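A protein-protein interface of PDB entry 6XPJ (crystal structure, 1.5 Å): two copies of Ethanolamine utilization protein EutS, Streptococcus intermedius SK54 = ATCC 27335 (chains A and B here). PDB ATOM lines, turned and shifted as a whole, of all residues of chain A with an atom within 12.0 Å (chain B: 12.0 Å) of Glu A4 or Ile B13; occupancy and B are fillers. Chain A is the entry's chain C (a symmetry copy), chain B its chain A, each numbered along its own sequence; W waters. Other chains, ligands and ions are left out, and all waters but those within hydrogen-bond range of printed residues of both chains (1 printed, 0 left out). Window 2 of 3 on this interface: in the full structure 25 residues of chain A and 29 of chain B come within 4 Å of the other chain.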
ATOM      1  N   GLY A   1     -22.256   2.889 -36.071  1.00  0.00           N
ATOM      2  CA  GLY A   1     -20.827   3.090 -36.425  1.00  0.00           C
ATOM      3  C   GLY A   1     -19.990   1.901 -35.994  1.00  0.00           C
ATOM      4  O   GLY A   1     -20.544   1.023 -35.318  1.00  0.00           O
ATOM      5  N   MET A   2     -18.716   1.873 -36.379  1.00  0.00           N
ATOM      6  CA  MET A   2     -17.791   0.731 -36.154  1.00  0.00           C
ATOM      7  C   MET A   2     -17.609   0.475 -34.646  1.00  0.00           C
ATOM      8  O   MET A   2     -17.688  -0.688 -34.227  1.00  0.00           O
ATOM      9  CB  MET A   2     -16.440   1.030 -36.816  1.00  0.00           C
ATOM     10  CG  MET A   2     -15.428  -0.090 -36.721  1.00  0.00           C
ATOM     11  SD  MET A   2     -15.855  -1.523 -37.748  1.00  0.00           S
ATOM     12  CE  MET A   2     -15.507  -0.888 -39.391  1.00  0.00           C
ATOM     13  N   ILE A   3     -17.347   1.508 -33.840  1.00  0.00           N
ATOM     14  CA  ILE A   3     -17.128   1.339 -32.373  1.00  0.00           C
ATOM     15  C   ILE A   3     -18.340   0.627 -31.757  1.00  0.00           C
ATOM     16  O   ILE A   3     -18.151  -0.320 -30.949  1.00  0.00           O
ATOM     17  CB  ILE A   3     -16.864   2.697 -31.696  1.00  0.00           C
ATOM     18  CG1 ILE A   3     -15.562   3.322 -32.221  1.00  0.00           C
ATOM     19  CG2 ILE A   3     -16.867   2.570 -30.169  1.00  0.00           C
ATOM     20  CD1 ILE A   3     -15.378   4.757 -31.847  1.00  0.00           C
ATOM     21  N   GLU A   4     -19.542   1.100 -32.094  1.00  0.00           N
ATOM     22  CA  GLU A   4     -20.833   0.602 -31.549  1.00  0.00           C
ATOM     23  C   GLU A   4     -21.072  -0.832 -32.039  1.00  0.00           C
ATOM     24  O   GLU A   4     -21.467  -1.698 -31.225  1.00  0.00           O
ATOM     25  CB  GLU A   4     -21.913   1.588 -32.004  1.00  0.00           C
ATOM     26  CG  GLU A   4     -23.338   1.217 -31.644  1.00  0.00           C
ATOM     27  CD  GLU A   4     -24.308   2.267 -32.157  1.00  0.00           C
ATOM     28  OE1 GLU A   4     -23.822   3.320 -32.597  1.00  0.00           O
ATOM     29  OE2 GLU A   4     -25.524   2.020 -32.141  1.00  0.00           O
ATOM     30  N   GLU A   5     -20.881  -1.073 -33.338  1.00  0.00           N
ATOM     31  CA  GLU A   5     -21.158  -2.395 -33.955  1.00  0.00           C
ATOM     32  C   GLU A   5     -20.204  -3.431 -33.345  1.00  0.00           C
ATOM     33  O   GLU A   5     -20.671  -4.512 -32.930  1.00  0.00           O
ATOM     34  CB  GLU A   5     -21.056  -2.304 -35.482  1.00  0.00           C
ATOM     35  CG  GLU A   5     -22.281  -1.670 -36.132  1.00  0.00           C
ATOM     36  CD  GLU A   5     -23.609  -2.244 -35.661  1.00  0.00           C
ATOM     37  OE1 GLU A   5     -23.893  -3.418 -35.983  1.00  0.00           O
ATOM     38  OE2 GLU A   5     -24.343  -1.526 -34.937  1.00  0.00           O
ATOM     39  N   LEU A   6     -18.909  -3.132 -33.263  1.00  0.00           N
ATOM     40  CA  LEU A   6     -17.922  -4.183 -32.884  1.00  0.00           C
ATOM     41  C   LEU A   6     -17.870  -4.330 -31.362  1.00  0.00           C
ATOM     42  O   LEU A   6     -17.515  -5.437 -30.877  1.00  0.00           O
ATOM     43  CB  LEU A   6     -16.585  -3.851 -33.543  1.00  0.00           C
ATOM     44  CG  LEU A   6     -16.615  -4.094 -35.051  1.00  0.00           C
ATOM     45  CD1 LEU A   6     -15.337  -3.657 -35.694  1.00  0.00           C
ATOM     46  CD2 LEU A   6     -16.870  -5.556 -35.374  1.00  0.00           C
ATOM     47  N   GLY A   7     -18.321  -3.308 -30.633  1.00  0.00           N
ATOM     48  CA  GLY A   7     -18.448  -3.365 -29.166  1.00  0.00           C
ATOM     49  C   GLY A   7     -19.777  -3.978 -28.742  1.00  0.00           C
ATOM     50  O   GLY A   7     -19.935  -4.221 -27.534  1.00  0.00           O
ATOM     51  N   LYS A   8     -20.699  -4.205 -29.691  1.00  0.00           N
ATOM     52  CA  LYS A   8     -22.099  -4.676 -29.462  1.00  0.00           C
ATOM     53  C   LYS A   8     -22.718  -3.808 -28.356  1.00  0.00           C
ATOM     54  O   LYS A   8     -23.273  -4.351 -27.381  1.00  0.00           O
ATOM     55  CB  LYS A   8     -22.148  -6.177 -29.143  1.00  0.00           C
ATOM     56  CG  LYS A   8     -21.691  -7.068 -30.292  1.00  0.00           C
ATOM     57  CD  LYS A   8     -22.254  -8.476 -30.264  1.00  0.00           C
ATOM     58  CE  LYS A   8     -21.470  -9.413 -29.372  1.00  0.00           C
ATOM     59  NZ  LYS A   8     -22.024 -10.789 -29.411  1.00  0.00           N
ATOM     60  N   ILE A   9     -22.612  -2.490 -28.519  1.00  0.00           N
ATOM     61  CA  ILE A   9     -23.184  -1.492 -27.569  1.00  0.00           C
ATOM     62  C   ILE A   9     -24.636  -1.233 -27.990  1.00  0.00           C
ATOM     63  O   ILE A   9     -24.853  -0.830 -29.142  1.00  0.00           O
ATOM     64  CB  ILE A   9     -22.336  -0.207 -27.562  1.00  0.00           C
ATOM     65  CG1 ILE A   9     -20.838  -0.526 -27.472  1.00  0.00           C
ATOM     66  CG2 ILE A   9     -22.786   0.712 -26.432  1.00  0.00           C
ATOM     67  CD1 ILE A   9     -19.932   0.676 -27.310  1.00  0.00           C
ATOM     68  N   ASP A  10     -25.591  -1.472 -27.092  1.00  0.00           N
ATOM     69  CA  ASP A  10     -27.025  -1.232 -27.363  1.00  0.00           C
ATOM     70  C   ASP A  10     -27.315   0.261 -27.238  1.00  0.00           C
ATOM     71  O   ASP A  10     -26.491   0.990 -26.657  1.00  0.00           O
ATOM     72  CB  ASP A  10     -27.918  -2.020 -26.413  1.00  0.00           C
ATOM     73  CG  ASP A  10     -27.828  -3.512 -26.659  1.00  0.00           C
ATOM     74  OD1 ASP A  10     -28.021  -3.924 -27.820  1.00  0.00           O
ATOM     75  OD2 ASP A  10     -27.510  -4.233 -25.701  1.00  0.00           O
ATOM     76  N   ARG A  11     -28.463   0.646 -27.743  1.00  0.00           N
ATOM     77  CA  ARG A  11     -28.901   2.051 -27.839  1.00  0.00           C
ATOM     78  C   ARG A  11     -30.333   2.114 -27.304  1.00  0.00           C
ATOM     79  O   ARG A  11     -31.136   1.238 -27.671  1.00  0.00           O
ATOM     80  CB  ARG A  11     -28.687   2.457 -29.294  1.00  0.00           C
ATOM     81  CG  ARG A  11     -28.939   3.910 -29.622  1.00  0.00           C
ATOM     82  CD  ARG A  11     -28.627   4.162 -31.083  1.00  0.00           C
ATOM     83  NE  ARG A  11     -27.227   4.347 -31.429  1.00  0.00           N
ATOM     84  CZ  ARG A  11     -26.618   5.530 -31.562  1.00  0.00           C
ATOM     85  NH1 ARG A  11     -27.258   6.679 -31.362  1.00  0.00           N
ATOM     86  NH2 ARG A  11     -25.346   5.562 -31.907  1.00  0.00           N
ATOM     87  N   ILE A  12     -30.628   3.088 -26.439  1.00  0.00           N
ATOM     88  CA  ILE A  12     -31.996   3.330 -25.904  1.00  0.00           C
ATOM     89  C   ILE A  12     -32.250   4.834 -25.979  1.00  0.00           C
ATOM     90  O   ILE A  12     -31.297   5.633 -25.815  1.00  0.00           O
ATOM     91  CB  ILE A  12     -32.146   2.805 -24.461  1.00  0.00           C
ATOM     92  CG1 ILE A  12     -33.591   2.827 -23.954  1.00  0.00           C
ATOM     93  CG2 ILE A  12     -31.222   3.513 -23.505  1.00  0.00           C
ATOM     94  CD1 ILE A  12     -33.806   1.966 -22.727  1.00  0.00           C
ATOM     95  N   ILE A  13     -33.495   5.226 -26.167  1.00  0.00           N
ATOM     96  CA  ILE A  13     -33.903   6.648 -26.024  1.00  0.00           C
ATOM     97  C   ILE A  13     -34.263   6.883 -24.568  1.00  0.00           C
ATOM     98  O   ILE A  13     -35.101   6.131 -24.005  1.00  0.00           O
ATOM     99  CB  ILE A  13     -35.066   7.001 -26.963  1.00  0.00           C
ATOM    100  CG1 ILE A  13     -34.684   6.794 -28.435  1.00  0.00           C
ATOM    101  CG2 ILE A  13     -35.520   8.427 -26.678  1.00  0.00           C
ATOM    102  CD1 ILE A  13     -35.867   6.780 -29.356  1.00  0.00           C
ATOM    103  N   GLN A  14     -33.700   7.931 -23.974  1.00  0.00           N
ATOM    104  CA  GLN A  14     -34.055   8.306 -22.587  1.00  0.00           C
ATOM    105  C   GLN A  14     -34.676   9.692 -22.588  1.00  0.00           C
ATOM    106  O   GLN A  14     -34.018  10.644 -23.006  1.00  0.00           O
ATOM    107  CB  GLN A  14     -32.850   8.236 -21.667  1.00  0.00           C
ATOM    108  CG  GLN A  14     -32.416   6.807 -21.447  1.00  0.00           C
ATOM    109  CD  GLN A  14     -31.561   6.657 -20.216  1.00  0.00           C
ATOM    110  OE1 GLN A  14     -31.055   7.629 -19.659  1.00  0.00           O
ATOM    111  NE2 GLN A  14     -31.403   5.424 -19.769  1.00  0.00           N
ATOM    112  N   GLU A  15     -35.939   9.743 -22.170  1.00  0.00           N
ATOM    113  CA  GLU A  15     -36.665  11.015 -21.994  1.00  0.00           C
ATOM    114  C   GLU A  15     -36.306  11.546 -20.625  1.00  0.00           C
ATOM    115  O   GLU A  15     -36.749  10.955 -19.607  1.00  0.00           O
ATOM    116  CB  GLU A  15     -38.181  10.849 -22.076  1.00  0.00           C
ATOM    117  CG  GLU A  15     -38.649  10.406 -23.422  1.00  0.00           C
ATOM    118  CD  GLU A  15     -40.164  10.450 -23.551  1.00  0.00           C
ATOM    119  OE1 GLU A  15     -40.865  10.720 -22.555  1.00  0.00           O
ATOM    120  OE2 GLU A  15     -40.611  10.148 -24.607  1.00  0.00           O
ATOM    121  N   ILE B   9     -19.038  -3.449 -15.014  1.00  0.00           N
ATOM    122  CA  ILE B   9     -20.139  -2.446 -15.222  1.00  0.00           C
ATOM    123  C   ILE B   9     -20.382  -2.294 -16.728  1.00  0.00           C
ATOM    124  O   ILE B   9     -19.419  -1.980 -17.457  1.00  0.00           O
ATOM    125  CB  ILE B   9     -19.795  -1.103 -14.543  1.00  0.00           C
ATOM    126  CG1 ILE B   9     -19.816  -1.221 -13.015  1.00  0.00           C
ATOM    127  CG2 ILE B   9     -20.715   0.008 -15.028  1.00  0.00           C
ATOM    128  CD1 ILE B   9     -18.973  -0.186 -12.308  1.00  0.00           C
ATOM    129  N   ASP B  10     -21.619  -2.507 -17.185  1.00  0.00           N
ATOM    130  CA  ASP B  10     -21.930  -2.518 -18.635  1.00  0.00           C
ATOM    131  C   ASP B  10     -22.068  -1.072 -19.112  1.00  0.00           C
ATOM    132  O   ASP B  10     -22.055  -0.153 -18.288  1.00  0.00           O
ATOM    133  CB  ASP B  10     -23.134  -3.377 -19.031  1.00  0.00           C
ATOM    134  CG  ASP B  10     -24.098  -3.732 -17.924  1.00  0.00           C
ATOM    135  OD1 ASP B  10     -24.576  -2.798 -17.259  1.00  0.00           O
ATOM    136  OD2 ASP B  10     -24.363  -4.946 -17.747  1.00  0.00           O
ATOM    137  N   ARG B  11     -22.078  -0.915 -20.418  1.00  0.00           N
ATOM    138  CA  ARG B  11     -22.144   0.388 -21.119  1.00  0.00           C
ATOM    139  C   ARG B  11     -23.310   0.310 -22.106  1.00  0.00           C
ATOM    140  O   ARG B  11     -23.465  -0.709 -22.803  1.00  0.00           O
ATOM    141  CB  ARG B  11     -20.775   0.644 -21.758  1.00  0.00           C
ATOM    142  CG  ARG B  11     -20.679   1.866 -22.649  1.00  0.00           C
ATOM    143  CD  ARG B  11     -19.311   1.880 -23.328  1.00  0.00           C
ATOM    144  NE  ARG B  11     -18.225   2.115 -22.387  1.00  0.00           N
ATOM    145  CZ  ARG B  11     -17.620   3.293 -22.151  1.00  0.00           C
ATOM    146  NH1 ARG B  11     -17.975   4.364 -22.823  1.00  0.00           N
ATOM    147  NH2 ARG B  11     -16.631   3.367 -21.261  1.00  0.00           N
ATOM    148  N   ILE B  12     -24.121   1.344 -22.137  1.00  0.00           N
ATOM    149  CA  ILE B  12     -25.223   1.496 -23.128  1.00  0.00           C
ATOM    150  C   ILE B  12     -25.139   2.902 -23.702  1.00  0.00           C
ATOM    151  O   ILE B  12     -24.720   3.813 -22.985  1.00  0.00           O
ATOM    152  CB  ILE B  12     -26.601   1.204 -22.497  1.00  0.00           C
ATOM    153  CG1 ILE B  12     -27.705   1.115 -23.556  1.00  0.00           C
ATOM    154  CG2 ILE B  12     -26.957   2.208 -21.440  1.00  0.00           C
ATOM    155  CD1 ILE B  12     -28.922   0.323 -23.101  1.00  0.00           C
ATOM    156  N   ILE B  13     -25.562   3.081 -24.936  1.00  0.00           N
ATOM    157  CA  ILE B  13     -25.721   4.419 -25.564  1.00  0.00           C
ATOM    158  C   ILE B  13     -27.129   4.897 -25.220  1.00  0.00           C
ATOM    159  O   ILE B  13     -28.096   4.155 -25.464  1.00  0.00           O
ATOM    160  CB  ILE B  13     -25.476   4.401 -27.088  1.00  0.00           C
ATOM    161  CG1 ILE B  13     -24.047   3.969 -27.428  1.00  0.00           C
ATOM    162  CG2 ILE B  13     -25.809   5.749 -27.711  1.00  0.00           C
ATOM    163  CD1 ILE B  13     -23.927   3.357 -28.790  1.00  0.00           C
ATOM    164  N   GLN B  14     -27.213   6.100 -24.683  1.00  0.00           N
ATOM    165  CA  GLN B  14     -28.445   6.815 -24.265  1.00  0.00           C
ATOM    166  C   GLN B  14     -28.684   7.952 -25.261  1.00  0.00           C
ATOM    167  O   GLN B  14     -27.900   8.883 -25.178  1.00  0.00           O
ATOM    168  CB  GLN B  14     -28.191   7.368 -22.853  1.00  0.00           C
ATOM    169  CG  GLN B  14     -29.125   8.466 -22.352  1.00  0.00           C
ATOM    170  CD  GLN B  14     -28.356   9.605 -21.721  1.00  0.00           C
ATOM    171  OE1 GLN B  14     -28.074   9.617 -20.524  1.00  0.00           O
ATOM    172  NE2 GLN B  14     -27.976  10.560 -22.552  1.00  0.00           N
ATOM    173  N   GLU B  15     -29.701   7.898 -26.118  1.00  0.00           N
ATOM    174  CA  GLU B  15     -30.104   9.062 -26.919  1.00  0.00           C
ATOM    175  C   GLU B  15     -30.948   9.949 -26.014  1.00  0.00           C
ATOM    176  O   GLU B  15     -32.088   9.562 -25.709  1.00  0.00           O
ATOM    177  CB  GLU B  15     -30.882   8.653 -28.165  1.00  0.00           C
ATOM    178  CG  GLU B  15     -30.045   7.871 -29.120  1.00  0.00           C
ATOM    179  CD  GLU B  15     -30.737   7.573 -30.432  1.00  0.00           C
ATOM    180  OE1 GLU B  15     -31.847   8.061 -30.627  1.00  0.00           O
ATOM    181  OE2 GLU B  15     -30.156   6.840 -31.251  1.00  0.00           O
ATOM    182  N   SER B  16     -30.421  11.108 -25.641  1.00  0.00           N
ATOM    183  CA  SER B  16     -31.043  12.029 -24.672  1.00  0.00           C
ATOM    184  C   SER B  16     -32.029  12.941 -25.388  1.00  0.00           C
ATOM    185  O   SER B  16     -31.632  13.704 -26.278  1.00  0.00           O
ATOM    186  CB  SER B  16     -29.995  12.794 -23.954  1.00  0.00           C
ATOM    187  OG  SER B  16     -30.542  13.465 -22.835  1.00  0.00           O
ATOM    188  N   VAL B  17     -33.258  12.947 -24.916  1.00  0.00           N
ATOM    189  CA  VAL B  17     -34.285  13.905 -25.393  1.00  0.00           C
ATOM    190  C   VAL B  17     -34.993  14.409 -24.150  1.00  0.00           C
ATOM    191  O   VAL B  17     -35.025  13.723 -23.133  1.00  0.00           O
ATOM    192  CB  VAL B  17     -35.257  13.258 -26.398  1.00  0.00           C
ATOM    193  CG1 VAL B  17     -34.506  12.688 -27.612  1.00  0.00           C
ATOM    194  CG2 VAL B  17     -36.115  12.184 -25.757  1.00  0.00           C
HETATM  195  O   HOH W   1     -24.865  -2.263 -24.427  1.00  0.00           O
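Hydrophobic or aromatic side chains of chain A within 4 Å of the printed part of chain B: Ile A9, Ile A12 and Ile A13. Printed residues of chain B that touch a printed residue of chain A: Arg B11, Ile B12, Ile B13, Gln B14, Glu B15, Ser B16 and Val B17. Hydrophobic or aromatic side chains of chain B that line the printed part of chain A: Ile B12, Ile B13 and Val B17. Among the printed residues, Asp or Glu carboxylates within 4 Å of a Lys or Arg side-chain nitrogen of the other chain: Arg A11 with Glu B15 (2.9 Å).
Among the printed residues, merely in contact across the chains: Arg A11 with Ile B13 (3.3 Å), Asp A10 with Ile B12 (3.3 Å), Glu A15 with Val B17 (3.4 Å), Gln A14 with Gln B14 (3.4 Å), Ile A13 with Glu B15 (3.4 Å), Ile A12 with Gln B14 (3.5 Å), Glu A4 with Ile B13 (3.6 Å), Ile A9 with Ile B13 (3.6 Å), Gln A14 with Ser B16 (3.7 Å), Ile A13 with Val B17 (3.9 Å), Ile A12 with Ile B12 (3.95 Å) and Ile A9 with Arg B11 (3.96 Å).
Water W1 lies within hydrogen-bond range of the backbone carbonyl oxygen of Arg B11 (2.6 Å) and the backbone NH of Asp A10 (2.9 Å).
Printed residues of chain A within 4 Å of Ile B13: Glu A4, Ile A9, Asp A10, Arg A11 and Ile A12. No residue of chain B comes within 4 Å of Ile A3. No residue of chain B comes within 4 Å of Glu A5. No residue of chain B comes within 4 Å of Leu A6. Ile A9 touches just these residues of chain B: Arg B11 (3.96 Å) and Ile B13 (3.6 Å). Of the printed residues of chain B, Asp A10 touches Ile B12 (3.3 Å) and Ile B13 (2.9 Å). Of chain B, only Ile B13 (3.3 Å) and Glu B15 (2.9 Å) come within 4 Å of Arg A11. Printed residues of chain A within 4 Å of Ile B12: Asp A10 (3.3 Å) and Ile A12 (3.95 Å). Printed residues of chain A within 4 Å of Gln B14: Ile A12 (3.5 Å) and Gln A14 (3.4 Å). Of the printed residues of chain A, Arg B11 touches Ile A9 (3.96 Å). Printed residues of chain B within 4 Å of Gln A14: Gln B14, Glu B15, Ser B16 and Val B17. Of the printed residues of chain A, Glu B15 touches Arg A11 (2.9 Å), Ile A12 (2.8 Å), Ile A13 (3.4 Å) and Gln A14 (2.9 Å). Printed residues of chain B within 4 Å of Ile A12: Ile B12 (3.95 Å), Ile B13 (2.9 Å), Gln B14 (3.5 Å) and Glu B15 (2.8 Å). Ile B9 touches none of the printed residues of chain A. Asp B10 touches none of the printed residues of chain A. The nearest residue of chain B that does not touch Glu A4 is Glu B15 (6.7 Å).
The backbone NH (N) of Ile B13 is in hydrogen-bond range of the backbone carbonyl oxygen (O) of Asp A10 (2.9 Å). N of Ile A12 sits at hydrogen-bond distance from O of Ile B13 (2.9 Å). OE2 of Glu B15 lies within salt-bridge range of NH1 of Arg A11 (2.9 Å). The backbone NH (N) of Glu B15 sits at hydrogen-bond distance from the backbone carbonyl oxygen (O) of Ile A12. The backbone carbonyl oxygen of Glu B15 lies within hydrogen-bond range of the backbone NH of Gln A14 (2.9 Å). The backbone NH of Val B17 sits at hydrogen-bond distance from the backbone carbonyl oxygen of Gln A14 (3.1 Å).
O of Glu A4 is in hydrogen-bond range of N of Ile A9 (3.0 Å). OE1 of Glu A4 lies within salt-bridge range of NH2 of Arg A11, 2.8 Å away.
Arg A11 touches Ile B13, but with the chains exchanged Ile A13 does not touch Arg B11 (12.0 Å). Arg A11 touches Glu B15, but with the chains exchanged Glu A15 does not touch Arg B11 (15.8 Å). Gln A14 touches its own counterpart, Gln B14. Gln A14 touches Glu B15, but with the chains exchanged Glu A15 does not touch Gln B14 (6.9 Å). Positions printed for both chains: 9, 10, 11, 12, 13, 14 and 15.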
